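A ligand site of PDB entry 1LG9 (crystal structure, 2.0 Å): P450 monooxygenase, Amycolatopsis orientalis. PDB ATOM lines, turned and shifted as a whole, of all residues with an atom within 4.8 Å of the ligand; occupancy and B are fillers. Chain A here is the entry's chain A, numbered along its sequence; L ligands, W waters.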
ATOM      1  N   MET A  55     -39.616  -0.853 -13.482  1.00  0.00           N
ATOM      2  CA  MET A  55     -38.569  -1.129 -14.479  1.00  0.00           C
ATOM      3  C   MET A  55     -39.017  -1.970 -15.677  1.00  0.00           C
ATOM      4  O   MET A  55     -38.514  -1.801 -16.765  1.00  0.00           O
ATOM      5  CB  MET A  55     -37.366  -1.838 -13.801  1.00  0.00           C
ATOM      6  CG  MET A  55     -36.617  -0.852 -12.889  1.00  0.00           C
ATOM      7  SD  MET A  55     -35.066  -1.511 -12.172  1.00  0.00           S
ATOM      8  CE  MET A  55     -33.978  -1.277 -13.546  1.00  0.00           C
ATOM      9  N   LEU A  88     -27.879   4.009 -24.611  1.00  0.00           N
ATOM     10  CA  LEU A  88     -29.109   3.193 -24.517  1.00  0.00           C
ATOM     11  C   LEU A  88     -30.078   3.530 -23.418  1.00  0.00           C
ATOM     12  O   LEU A  88     -31.285   3.410 -23.604  1.00  0.00           O
ATOM     13  CB  LEU A  88     -28.773   1.727 -24.337  1.00  0.00           C
ATOM     14  CG  LEU A  88     -27.991   1.119 -25.481  1.00  0.00           C
ATOM     15  CD1 LEU A  88     -27.824  -0.373 -25.230  1.00  0.00           C
ATOM     16  CD2 LEU A  88     -28.773   1.322 -26.768  1.00  0.00           C
ATOM     17  N   MET A  89     -29.580   3.978 -22.276  1.00  0.00           N
ATOM     18  CA  MET A  89     -30.444   4.241 -21.144  1.00  0.00           C
ATOM     19  C   MET A  89     -31.317   5.428 -21.383  1.00  0.00           C
ATOM     20  O   MET A  89     -32.339   5.552 -20.719  1.00  0.00           O
ATOM     21  CB  MET A  89     -29.632   4.425 -19.842  1.00  0.00           C
ATOM     22  CG  MET A  89     -29.108   3.077 -19.232  1.00  0.00           C
ATOM     23  SD  MET A  89     -27.874   3.251 -17.860  1.00  0.00           S
ATOM     24  CE  MET A  89     -26.339   3.638 -18.826  1.00  0.00           C
ATOM     25  N   HIS A  96     -35.179   2.557 -28.541  1.00  0.00           N
ATOM     26  CA  HIS A  96     -34.232   1.784 -27.752  1.00  0.00           C
ATOM     27  C   HIS A  96     -33.949   0.423 -28.377  1.00  0.00           C
ATOM     28  O   HIS A  96     -32.777   0.002 -28.456  1.00  0.00           O
ATOM     29  CB  HIS A  96     -34.778   1.528 -26.377  1.00  0.00           C
ATOM     30  CG  HIS A  96     -33.943   0.586 -25.566  1.00  0.00           C
ATOM     31  ND1 HIS A  96     -34.357  -0.685 -25.223  1.00  0.00           N
ATOM     32  CD2 HIS A  96     -32.716   0.765 -25.000  1.00  0.00           C
ATOM     33  CE1 HIS A  96     -33.430  -1.259 -24.480  1.00  0.00           C
ATOM     34  NE2 HIS A  96     -32.421  -0.402 -24.323  1.00  0.00           N
ATOM     35  N   ARG A 100     -30.262  -0.958 -29.257  1.00  0.00           N
ATOM     36  CA  ARG A 100     -29.709  -2.073 -28.489  1.00  0.00           C
ATOM     37  C   ARG A 100     -29.407  -3.256 -29.417  1.00  0.00           C
ATOM     38  O   ARG A 100     -28.372  -3.903 -29.298  1.00  0.00           O
ATOM     39  CB  ARG A 100     -30.638  -2.513 -27.345  1.00  0.00           C
ATOM     40  CG  ARG A 100     -30.041  -3.688 -26.510  1.00  0.00           C
ATOM     41  CD  ARG A 100     -30.803  -3.851 -25.212  1.00  0.00           C
ATOM     42  NE  ARG A 100     -30.396  -5.058 -24.515  1.00  0.00           N
ATOM     43  CZ  ARG A 100     -30.022  -5.118 -23.246  1.00  0.00           C
ATOM     44  NH1 ARG A 100     -29.969  -4.050 -22.491  1.00  0.00           N
ATOM     45  NH2 ARG A 100     -29.748  -6.299 -22.726  1.00  0.00           N
ATOM     46  N   PHE A 107     -21.535  -8.139 -27.486  1.00  0.00           N
ATOM     47  CA  PHE A 107     -21.776  -8.701 -26.138  1.00  0.00           C
ATOM     48  C   PHE A 107     -22.354 -10.125 -26.062  1.00  0.00           C
ATOM     49  O   PHE A 107     -22.836 -10.516 -24.987  1.00  0.00           O
ATOM     50  CB  PHE A 107     -22.726  -7.788 -25.354  1.00  0.00           C
ATOM     51  CG  PHE A 107     -22.149  -6.473 -25.043  1.00  0.00           C
ATOM     52  CD1 PHE A 107     -22.250  -5.411 -25.962  1.00  0.00           C
ATOM     53  CD2 PHE A 107     -21.478  -6.271 -23.842  1.00  0.00           C
ATOM     54  CE1 PHE A 107     -21.700  -4.155 -25.672  1.00  0.00           C
ATOM     55  CE2 PHE A 107     -20.927  -5.028 -23.548  1.00  0.00           C
ATOM     56  CZ  PHE A 107     -21.038  -3.968 -24.467  1.00  0.00           C
ATOM     57  N   LEU A 152     -12.432  -3.383 -20.395  1.00  0.00           N
ATOM     58  CA  LEU A 152     -13.270  -2.614 -21.328  1.00  0.00           C
ATOM     59  C   LEU A 152     -12.427  -2.265 -22.580  1.00  0.00           C
ATOM     60  O   LEU A 152     -12.913  -2.350 -23.709  1.00  0.00           O
ATOM     61  CB  LEU A 152     -13.786  -1.377 -20.628  1.00  0.00           C
ATOM     62  CG  LEU A 152     -14.874  -1.684 -19.586  1.00  0.00           C
ATOM     63  CD1 LEU A 152     -15.042  -0.564 -18.619  1.00  0.00           C
ATOM     64  CD2 LEU A 152     -16.185  -2.012 -20.339  1.00  0.00           C
ATOM     65  N   LEU A 155     -12.413  -5.272 -24.656  1.00  0.00           N
ATOM     66  CA  LEU A 155     -13.742  -5.434 -25.278  1.00  0.00           C
ATOM     67  C   LEU A 155     -13.990  -4.484 -26.476  1.00  0.00           C
ATOM     68  O   LEU A 155     -14.500  -4.879 -27.529  1.00  0.00           O
ATOM     69  CB  LEU A 155     -14.848  -5.177 -24.232  1.00  0.00           C
ATOM     70  CG  LEU A 155     -16.309  -5.076 -24.720  1.00  0.00           C
ATOM     71  CD1 LEU A 155     -16.905  -6.419 -25.024  1.00  0.00           C
ATOM     72  CD2 LEU A 155     -17.117  -4.340 -23.639  1.00  0.00           C
ATOM     73  N   VAL A 233     -20.265   2.647 -22.784  1.00  0.00           N
ATOM     74  CA  VAL A 233     -19.787   1.369 -22.339  1.00  0.00           C
ATOM     75  C   VAL A 233     -18.611   1.645 -21.368  1.00  0.00           C
ATOM     76  O   VAL A 233     -18.489   0.993 -20.294  1.00  0.00           O
ATOM     77  CB  VAL A 233     -19.325   0.548 -23.560  1.00  0.00           C
ATOM     78  CG1 VAL A 233     -18.393  -0.598 -23.148  1.00  0.00           C
ATOM     79  CG2 VAL A 233     -20.536   0.003 -24.292  1.00  0.00           C
ATOM     80  N   ALA A 236     -20.379   2.697 -18.254  1.00  0.00           N
ATOM     81  CA  ALA A 236     -21.226   1.714 -17.624  1.00  0.00           C
ATOM     82  C   ALA A 236     -20.491   0.548 -16.973  1.00  0.00           C
ATOM     83  O   ALA A 236     -21.003  -0.068 -16.051  1.00  0.00           O
ATOM     84  CB  ALA A 236     -22.248   1.165 -18.631  1.00  0.00           C
ATOM     85  N   GLY A 237     -19.305   0.192 -17.443  1.00  0.00           N
ATOM     86  CA  GLY A 237     -18.711  -0.981 -16.850  1.00  0.00           C
ATOM     87  C   GLY A 237     -17.464  -0.746 -16.021  1.00  0.00           C
ATOM     88  O   GLY A 237     -16.624  -1.683 -15.878  1.00  0.00           O
ATOM     89  N   ASN A 240     -19.096   0.228 -11.408  1.00  0.00           N
ATOM     90  CA  ASN A 240     -19.815  -0.902 -10.833  1.00  0.00           C
ATOM     91  C   ASN A 240     -18.891  -2.105 -10.581  1.00  0.00           C
ATOM     92  O   ASN A 240     -19.027  -2.819  -9.602  1.00  0.00           O
ATOM     93  CB  ASN A 240     -20.933  -1.342 -11.797  1.00  0.00           C
ATOM     94  CG  ASN A 240     -22.113  -0.364 -11.799  1.00  0.00           C
ATOM     95  OD1 ASN A 240     -22.292   0.374 -10.833  1.00  0.00           O
ATOM     96  ND2 ASN A 240     -22.914  -0.359 -12.887  1.00  0.00           N
ATOM     97  N   ILE A 241     -17.956  -2.335 -11.489  1.00  0.00           N
ATOM     98  CA  ILE A 241     -17.019  -3.436 -11.352  1.00  0.00           C
ATOM     99  C   ILE A 241     -15.954  -3.133 -10.315  1.00  0.00           C
ATOM    100  O   ILE A 241     -15.622  -4.022  -9.536  1.00  0.00           O
ATOM    101  CB  ILE A 241     -16.312  -3.771 -12.694  1.00  0.00           C
ATOM    102  CG1 ILE A 241     -17.361  -4.195 -13.720  1.00  0.00           C
ATOM    103  CG2 ILE A 241     -15.261  -4.927 -12.454  1.00  0.00           C
ATOM    104  CD1 ILE A 241     -17.999  -5.600 -13.423  1.00  0.00           C
ATOM    105  N   MET A 244     -17.521  -3.667  -7.005  1.00  0.00           N
ATOM    106  CA  MET A 244     -17.747  -5.084  -6.695  1.00  0.00           C
ATOM    107  C   MET A 244     -16.467  -5.798  -6.382  1.00  0.00           C
ATOM    108  O   MET A 244     -16.455  -6.692  -5.559  1.00  0.00           O
ATOM    109  CB  MET A 244     -18.431  -5.813  -7.866  1.00  0.00           C
ATOM    110  CG  MET A 244     -19.927  -5.749  -7.853  1.00  0.00           C
ATOM    111  SD  MET A 244     -20.695  -6.334  -6.348  1.00  0.00           S
ATOM    112  CE  MET A 244     -20.299  -8.051  -6.408  1.00  0.00           C
ATOM    113  N   VAL A 282     -24.147  -2.905  -5.806  1.00  0.00           N
ATOM    114  CA  VAL A 282     -23.399  -1.659  -5.761  1.00  0.00           C
ATOM    115  C   VAL A 282     -24.095  -0.458  -6.369  1.00  0.00           C
ATOM    116  O   VAL A 282     -23.895   0.625  -5.888  1.00  0.00           O
ATOM    117  CB  VAL A 282     -21.997  -1.770  -6.398  1.00  0.00           C
ATOM    118  CG1 VAL A 282     -21.121  -2.717  -5.615  1.00  0.00           C
ATOM    119  CG2 VAL A 282     -22.144  -2.259  -7.820  1.00  0.00           C
ATOM    120  N   PRO A 283     -24.956  -0.636  -7.387  1.00  0.00           N
ATOM    121  CA  PRO A 283     -25.593   0.590  -7.914  1.00  0.00           C
ATOM    122  C   PRO A 283     -26.698   1.037  -6.955  1.00  0.00           C
ATOM    123  O   PRO A 283     -27.526   0.241  -6.587  1.00  0.00           O
ATOM    124  CB  PRO A 283     -26.203   0.149  -9.256  1.00  0.00           C
ATOM    125  CG  PRO A 283     -25.709  -1.351  -9.484  1.00  0.00           C
ATOM    126  CD  PRO A 283     -25.491  -1.846  -8.056  1.00  0.00           C
ATOM    127  N   PRO A 286     -31.248   2.661 -10.688  1.00  0.00           N
ATOM    128  CA  PRO A 286     -31.090   2.678 -12.140  1.00  0.00           C
ATOM    129  C   PRO A 286     -31.525   4.076 -12.610  1.00  0.00           C
ATOM    130  O   PRO A 286     -31.743   4.965 -11.786  1.00  0.00           O
ATOM    131  CB  PRO A 286     -32.050   1.577 -12.591  1.00  0.00           C
ATOM    132  CG  PRO A 286     -33.234   1.786 -11.628  1.00  0.00           C
ATOM    133  CD  PRO A 286     -32.558   2.113 -10.285  1.00  0.00           C
ATOM    134  N   THR A 287     -31.596   4.269 -13.905  1.00  0.00           N
ATOM    135  CA  THR A 287     -32.026   5.553 -14.476  1.00  0.00           C
ATOM    136  C   THR A 287     -33.409   5.874 -13.880  1.00  0.00           C
ATOM    137  O   THR A 287     -34.245   4.993 -13.803  1.00  0.00           O
ATOM    138  CB  THR A 287     -32.192   5.412 -16.019  1.00  0.00           C
ATOM    139  OG1 THR A 287     -31.079   4.688 -16.561  1.00  0.00           O
ATOM    140  CG2 THR A 287     -32.296   6.758 -16.693  1.00  0.00           C
ATOM    141  N   ARG A 289     -37.251   6.663 -13.568  1.00  0.00           N
ATOM    142  CA  ARG A 289     -38.336   6.380 -14.500  1.00  0.00           C
ATOM    143  C   ARG A 289     -39.393   7.498 -14.415  1.00  0.00           C
ATOM    144  O   ARG A 289     -39.699   7.998 -13.327  1.00  0.00           O
ATOM    145  CB  ARG A 289     -39.027   5.048 -14.193  1.00  0.00           C
ATOM    146  CG  ARG A 289     -38.143   3.794 -14.235  1.00  0.00           C
ATOM    147  CD  ARG A 289     -37.082   3.816 -15.268  1.00  0.00           C
ATOM    148  NE  ARG A 289     -36.760   2.500 -15.845  1.00  0.00           N
ATOM    149  CZ  ARG A 289     -35.550   1.943 -15.808  1.00  0.00           C
ATOM    150  NH1 ARG A 289     -34.535   2.561 -15.199  1.00  0.00           N
ATOM    151  NH2 ARG A 289     -35.320   0.830 -16.484  1.00  0.00           N
ATOM    152  N   LEU A 312     -32.298  -0.313  -5.745  1.00  0.00           N
ATOM    153  CA  LEU A 312     -31.980  -1.700  -6.063  1.00  0.00           C
ATOM    154  C   LEU A 312     -31.503  -2.426  -4.813  1.00  0.00           C
ATOM    155  O   LEU A 312     -31.924  -3.560  -4.587  1.00  0.00           O
ATOM    156  CB  LEU A 312     -30.924  -1.792  -7.196  1.00  0.00           C
ATOM    157  CG  LEU A 312     -31.304  -1.025  -8.449  1.00  0.00           C
ATOM    158  CD1 LEU A 312     -30.176  -1.118  -9.516  1.00  0.00           C
ATOM    159  CD2 LEU A 312     -32.671  -1.598  -8.983  1.00  0.00           C
ATOM    160  N   VAL A 338     -32.223  -7.886  -8.720  1.00  0.00           N
ATOM    161  CA  VAL A 338     -32.395  -6.808  -9.674  1.00  0.00           C
ATOM    162  C   VAL A 338     -31.158  -5.927  -9.719  1.00  0.00           C
ATOM    163  O   VAL A 338     -31.228  -4.814 -10.147  1.00  0.00           O
ATOM    164  CB  VAL A 338     -33.657  -5.955  -9.329  1.00  0.00           C
ATOM    165  CG1 VAL A 338     -34.925  -6.857  -9.549  1.00  0.00           C
ATOM    166  CG2 VAL A 338     -33.581  -5.420  -7.912  1.00  0.00           C
ATOM    167  N   ALA A 339     -29.998  -6.421  -9.297  1.00  0.00           N
ATOM    168  CA  ALA A 339     -28.767  -5.630  -9.348  1.00  0.00           C
ATOM    169  C   ALA A 339     -28.365  -5.291 -10.797  1.00  0.00           C
ATOM    170  O   ALA A 339     -27.718  -4.271 -11.029  1.00  0.00           O
ATOM    171  CB  ALA A 339     -27.652  -6.363  -8.635  1.00  0.00           C
ATOM    172  N   PHE A 340     -28.773  -6.111 -11.788  1.00  0.00           N
ATOM    173  CA  PHE A 340     -28.471  -5.786 -13.183  1.00  0.00           C
ATOM    174  C   PHE A 340     -29.729  -5.169 -13.785  1.00  0.00           C
ATOM    175  O   PHE A 340     -29.854  -5.074 -14.996  1.00  0.00           O
ATOM    176  CB  PHE A 340     -28.083  -7.066 -13.996  1.00  0.00           C
ATOM    177  CG  PHE A 340     -26.712  -7.595 -13.695  1.00  0.00           C
ATOM    178  CD1 PHE A 340     -26.512  -8.935 -13.345  1.00  0.00           C
ATOM    179  CD2 PHE A 340     -25.603  -6.777 -13.842  1.00  0.00           C
ATOM    180  CE1 PHE A 340     -25.254  -9.423 -13.143  1.00  0.00           C
ATOM    181  CE2 PHE A 340     -24.324  -7.278 -13.636  1.00  0.00           C
ATOM    182  CZ  PHE A 340     -24.136  -8.569 -13.292  1.00  0.00           C
ATOM    183  N   GLY A 341     -30.676  -4.712 -12.953  1.00  0.00           N
ATOM    184  CA  GLY A 341     -31.861  -4.131 -13.508  1.00  0.00           C
ATOM    185  C   GLY A 341     -32.912  -5.186 -13.825  1.00  0.00           C
ATOM    186  O   GLY A 341     -32.901  -6.322 -13.303  1.00  0.00           O
ATOM    187  N   VAL A 344     -36.362  -4.218 -20.487  1.00  0.00           N
ATOM    188  CA  VAL A 344     -35.556  -4.112 -21.704  1.00  0.00           C
ATOM    189  C   VAL A 344     -34.215  -3.478 -21.515  1.00  0.00           C
ATOM    190  O   VAL A 344     -33.280  -3.691 -22.332  1.00  0.00           O
ATOM    191  CB  VAL A 344     -36.334  -3.381 -22.825  1.00  0.00           C
ATOM    192  CG1 VAL A 344     -37.639  -4.143 -23.089  1.00  0.00           C
ATOM    193  CG2 VAL A 344     -36.527  -1.857 -22.456  1.00  0.00           C
ATOM    194  N   HIS A 345     -34.065  -2.702 -20.448  1.00  0.00           N
ATOM    195  CA  HIS A 345     -32.781  -2.098 -20.193  1.00  0.00           C
ATOM    196  C   HIS A 345     -31.808  -2.981 -19.353  1.00  0.00           C
ATOM    197  O   HIS A 345     -30.728  -2.507 -18.969  1.00  0.00           O
ATOM    198  CB  HIS A 345     -32.933  -0.745 -19.485  1.00  0.00           C
ATOM    199  CG  HIS A 345     -33.515   0.325 -20.358  1.00  0.00           C
ATOM    200  ND1 HIS A 345     -32.758   1.051 -21.250  1.00  0.00           N
ATOM    201  CD2 HIS A 345     -34.783   0.832 -20.433  1.00  0.00           C
ATOM    202  CE1 HIS A 345     -33.520   1.956 -21.853  1.00  0.00           C
ATOM    203  NE2 HIS A 345     -34.751   1.838 -21.367  1.00  0.00           N
ATOM    204  N   HIS A 346     -32.204  -4.210 -19.020  1.00  0.00           N
ATOM    205  CA  HIS A 346     -31.350  -5.129 -18.208  1.00  0.00           C
ATOM    206  C   HIS A 346     -29.896  -5.057 -18.696  1.00  0.00           C
ATOM    207  O   HIS A 346     -29.648  -5.222 -19.887  1.00  0.00           O
ATOM    208  CB  HIS A 346     -31.870  -6.578 -18.403  1.00  0.00           C
ATOM    209  CG  HIS A 346     -31.190  -7.595 -17.515  1.00  0.00           C
ATOM    210  ND1 HIS A 346     -30.038  -8.273 -17.892  1.00  0.00           N
ATOM    211  CD2 HIS A 346     -31.517  -8.069 -16.285  1.00  0.00           C
ATOM    212  CE1 HIS A 346     -29.697  -9.113 -16.935  1.00  0.00           C
ATOM    213  NE2 HIS A 346     -30.575  -9.007 -15.951  1.00  0.00           N
ATOM    214  N   CYS A 347     -28.953  -4.938 -17.772  1.00  0.00           N
ATOM    215  CA  CYS A 347     -27.524  -4.733 -18.112  1.00  0.00           C
ATOM    216  C   CYS A 347     -27.055  -5.514 -19.321  1.00  0.00           C
ATOM    217  O   CYS A 347     -27.055  -6.709 -19.296  1.00  0.00           O
ATOM    218  CB  CYS A 347     -26.635  -5.100 -16.913  1.00  0.00           C
ATOM    219  SG  CYS A 347     -24.932  -4.760 -17.185  1.00  0.00           S
ATOM    220  N   LEU A 348     -26.629  -4.802 -20.336  1.00  0.00           N
ATOM    221  CA  LEU A 348     -26.147  -5.437 -21.577  1.00  0.00           C
ATOM    222  C   LEU A 348     -24.796  -6.161 -21.260  1.00  0.00           C
ATOM    223  O   LEU A 348     -24.403  -7.123 -21.924  1.00  0.00           O
ATOM    224  CB  LEU A 348     -25.912  -4.301 -22.639  1.00  0.00           C
ATOM    225  CG  LEU A 348     -25.496  -4.654 -24.072  1.00  0.00           C
ATOM    226  CD1 LEU A 348     -26.546  -5.593 -24.669  1.00  0.00           C
ATOM    227  CD2 LEU A 348     -25.229  -3.353 -24.936  1.00  0.00           C
ATOM    228  N   GLY A 349     -24.111  -5.671 -20.216  1.00  0.00           N
ATOM    229  CA  GLY A 349     -22.800  -6.194 -19.852  1.00  0.00           C
ATOM    230  C   GLY A 349     -22.818  -7.240 -18.768  1.00  0.00           C
ATOM    231  O   GLY A 349     -21.750  -7.679 -18.288  1.00  0.00           O
ATOM    232  N   LEU A 352     -20.466 -10.275 -19.237  1.00  0.00           N
ATOM    233  CA  LEU A 352     -19.064  -9.876 -19.117  1.00  0.00           C
ATOM    234  C   LEU A 352     -18.775  -9.586 -17.619  1.00  0.00           C
ATOM    235  O   LEU A 352     -17.721  -9.943 -17.102  1.00  0.00           O
ATOM    236  CB  LEU A 352     -18.775  -8.592 -19.911  1.00  0.00           C
ATOM    237  CG  LEU A 352     -17.385  -7.915 -19.733  1.00  0.00           C
ATOM    238  CD1 LEU A 352     -16.305  -8.948 -20.141  1.00  0.00           C
ATOM    239  CD2 LEU A 352     -17.224  -6.696 -20.664  1.00  0.00           C
ATOM    240  N   ALA A 353     -19.694  -8.917 -16.931  1.00  0.00           N
ATOM    241  CA  ALA A 353     -19.488  -8.600 -15.507  1.00  0.00           C
ATOM    242  C   ALA A 353     -19.315  -9.898 -14.693  1.00  0.00           C
ATOM    243  O   ALA A 353     -18.382 -10.009 -13.890  1.00  0.00           O
ATOM    244  CB  ALA A 353     -20.646  -7.781 -14.955  1.00  0.00           C
ATOM    245  N   GLU A 356     -15.933 -11.409 -15.613  1.00  0.00           N
ATOM    246  CA  GLU A 356     -14.807 -10.621 -15.108  1.00  0.00           C
ATOM    247  C   GLU A 356     -14.595 -10.799 -13.588  1.00  0.00           C
ATOM    248  O   GLU A 356     -13.496 -11.073 -13.130  1.00  0.00           O
ATOM    249  CB  GLU A 356     -15.045  -9.129 -15.484  1.00  0.00           C
ATOM    250  CG  GLU A 356     -13.995  -8.226 -15.024  1.00  0.00           C
ATOM    251  CD  GLU A 356     -14.114  -6.747 -15.528  1.00  0.00           C
ATOM    252  OE1 GLU A 356     -13.187  -6.005 -15.179  1.00  0.00           O
ATOM    253  OE2 GLU A 356     -15.082  -6.336 -16.213  1.00  0.00           O
ATOM    254  N   LEU A 357     -15.685 -10.681 -12.820  1.00  0.00           N
ATOM    255  CA  LEU A 357     -15.664 -10.859 -11.375  1.00  0.00           C
ATOM    256  C   LEU A 357     -15.277 -12.316 -11.008  1.00  0.00           C
ATOM    257  O   LEU A 357     -14.476 -12.561 -10.104  1.00  0.00           O
ATOM    258  CB  LEU A 357     -17.030 -10.492 -10.799  1.00  0.00           C
ATOM    259  CG  LEU A 357     -17.306  -8.984 -10.887  1.00  0.00           C
ATOM    260  CD1 LEU A 357     -18.796  -8.762 -10.448  1.00  0.00           C
ATOM    261  CD2 LEU A 357     -16.377  -8.189  -9.931  1.00  0.00           C
HETATM  262  C1  LIG L   1     -27.372  -1.118 -17.690  1.00  0.00           C
HETATM  263  C2  LIG L   1     -25.893  -2.717 -13.365  1.00  0.00           C
HETATM  264  C3  LIG L   1     -21.654  -3.928 -15.393  1.00  0.00           C
HETATM  265  C4  LIG L   1     -23.005  -2.081 -19.637  1.00  0.00           C
HETATM  266  C5  LIG L   1     -27.445  -1.639 -16.440  1.00  0.00           C
HETATM  267  C6  LIG L   1     -28.501  -1.391 -15.494  1.00  0.00           C
HETATM  268  C7  LIG L   1     -28.063  -1.725 -14.247  1.00  0.00           C
HETATM  269  C8  LIG L   1     -26.673  -2.133 -14.431  1.00  0.00           C
HETATM  270  C9  LIG L   1     -28.869  -1.795 -12.893  1.00  0.00           C
HETATM  271  C10 LIG L   1     -29.948  -0.959 -15.814  1.00  0.00           C
HETATM  272  C11 LIG L   1     -30.153   0.552 -15.741  1.00  0.00           C
HETATM  273  C12 LIG L   1     -31.619   0.996 -15.983  1.00  0.00           C
HETATM  274  O1  LIG L   1     -31.832   2.237 -16.044  1.00  0.00           O
HETATM  275  O2  LIG L   1     -32.528   0.138 -16.111  1.00  0.00           O
HETATM  276  C13 LIG L   1     -24.625  -3.277 -13.575  1.00  0.00           C
HETATM  277  C14 LIG L   1     -23.806  -3.852 -12.482  1.00  0.00           C
HETATM  278  C15 LIG L   1     -22.665  -4.134 -13.023  1.00  0.00           C
HETATM  279  C16 LIG L   1     -22.716  -3.757 -14.433  1.00  0.00           C
HETATM  280  C17 LIG L   1     -24.380  -4.128 -11.014  1.00  0.00           C
HETATM  281  C18 LIG L   1     -21.474  -4.818 -12.470  1.00  0.00           C
HETATM  282  C19 LIG L   1     -21.382  -5.476 -11.328  1.00  0.00           C
HETATM  283  C20 LIG L   1     -21.604  -3.550 -16.737  1.00  0.00           C
HETATM  284  C21 LIG L   1     -20.468  -3.813 -17.671  1.00  0.00           C
HETATM  285  C22 LIG L   1     -20.904  -3.300 -18.907  1.00  0.00           C
HETATM  286  C23 LIG L   1     -22.241  -2.783 -18.708  1.00  0.00           C
HETATM  287  C24 LIG L   1     -19.178  -4.693 -17.270  1.00  0.00           C
HETATM  288  C25 LIG L   1     -20.170  -2.973 -20.052  1.00  0.00           C
HETATM  289  C26 LIG L   1     -19.397  -3.738 -20.847  1.00  0.00           C
HETATM  290  C27 LIG L   1     -24.311  -1.553 -19.433  1.00  0.00           C
HETATM  291  C28 LIG L   1     -25.082  -0.922 -20.460  1.00  0.00           C
HETATM  292  C29 LIG L   1     -26.300  -0.722 -19.964  1.00  0.00           C
HETATM  293  C30 LIG L   1     -26.302  -1.258 -18.621  1.00  0.00           C
HETATM  294  C31 LIG L   1     -24.550  -0.596 -21.898  1.00  0.00           C
HETATM  295  C32 LIG L   1     -27.499  -0.102 -20.727  1.00  0.00           C
HETATM  296  C33 LIG L   1     -28.512  -1.143 -21.245  1.00  0.00           C
HETATM  297  C34 LIG L   1     -29.780  -0.531 -21.861  1.00  0.00           C
HETATM  298  O3  LIG L   1     -30.413  -1.223 -22.711  1.00  0.00           O
HETATM  299  O4  LIG L   1     -30.155   0.619 -21.459  1.00  0.00           O
HETATM  300  N1  LIG L   1     -26.276  -2.075 -15.777  1.00  0.00           N
HETATM  301  N2  LIG L   1     -23.889  -3.197 -14.793  1.00  0.00           N
HETATM  302  N3  LIG L   1     -22.671  -2.959 -17.360  1.00  0.00           N
HETATM  303  N4  LIG L   1     -25.082  -1.755 -18.307  1.00  0.00           N
HETATM  304 FE1  LIG L   1     -24.484  -2.617 -16.597  1.00  0.00          FE
HETATM  305  O   HOH W   1     -23.679  -0.573 -15.849  1.00  0.00           O
HETATM  306  O   HOH W   2     -32.955  -2.566 -16.330  1.00  0.00           O
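Residues that only touch the ligand: Met 55, Leu 88, Met 89, Phe 107, Leu 152, Leu 155, Ala 236, Gly 237, Asn 240, Ile 241, Met 244, Pro 283, Pro 286, Leu 312, Ala 339, Phe 340, Gly 341, Val 344, Leu 348, Gly 349, Leu 352 and Ala 353. Along chain A the residues within 4 Å of the ligand span positions 55 to 353. The nearest printed residue that does not touch the ligand is Val 233 (4.02 Å).
A ring nitrogen (ND1) of His 345 is in hydrogen-bond range of a ring nitrogen (NE2) of His 96 (3.4 Å). The backbone carbonyl oxygen (O) of Phe 340 is in hydrogen-bond range of the backbone NH (N) of Cys 347 (2.9 Å). The side-chain sulfur of Met 89 sits close to the side-chain hydroxyl of Thr 287, 3.7 Å away. The guanidinium group of Arg 100 is in hydrogen-bond range of the backbone carbonyl oxygen of His 346 (2.9 Å). The guanidinium group (NH1) of Arg 100 lies within hydrogen-bond range of the backbone carbonyl oxygen (O) of Val 344. The guanidinium group (NH1) of Arg 289 sits at hydrogen-bond distance from the backbone carbonyl oxygen (O) of Thr 287 (2.8 Å). The side-chain sulfur of Cys 347 lies close to the backbone NH of Gly 349 (3.3 Å).
Water W1 lies within hydrogen-bond range of the backbone carbonyl oxygen (O) of Ala 236 and the side-chain amide nitrogen (ND2) of Asn 240. Water W2 lies within hydrogen-bond range of O2 of the ligand (2.7 Å), N of His 346 (3.2 Å) and O of His 345 (3.5 Å).
ND1 of His 345 lies within hydrogen-bond range of O4 of the ligand, 2.6 Å away. The backbone NH (N) of Thr 287 lies within hydrogen-bond range of an oxygen (O1) of the ligand (3.0 Å). The guanidinium group (NH1) of Arg 289 lies within salt-bridge range of an oxygen (O1) of the ligand (2.9 Å). NH1 of Arg 100 lies within salt-bridge range of O3 of the ligand, 2.9 Å away. An iron atom (FE1) of the ligand is bound by the side-chain sulfur (SG) of Cys 347, 2.3 Å away. An oxygen (O3) of the ligand lies within hydrogen-bond range of a ring nitrogen (NE2) of His 96, at 2.7 Å. The side-chain hydroxyl (OG1) of Thr 287 lies within hydrogen-bond range of an oxygen (O1) of the ligand (2.6 Å).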
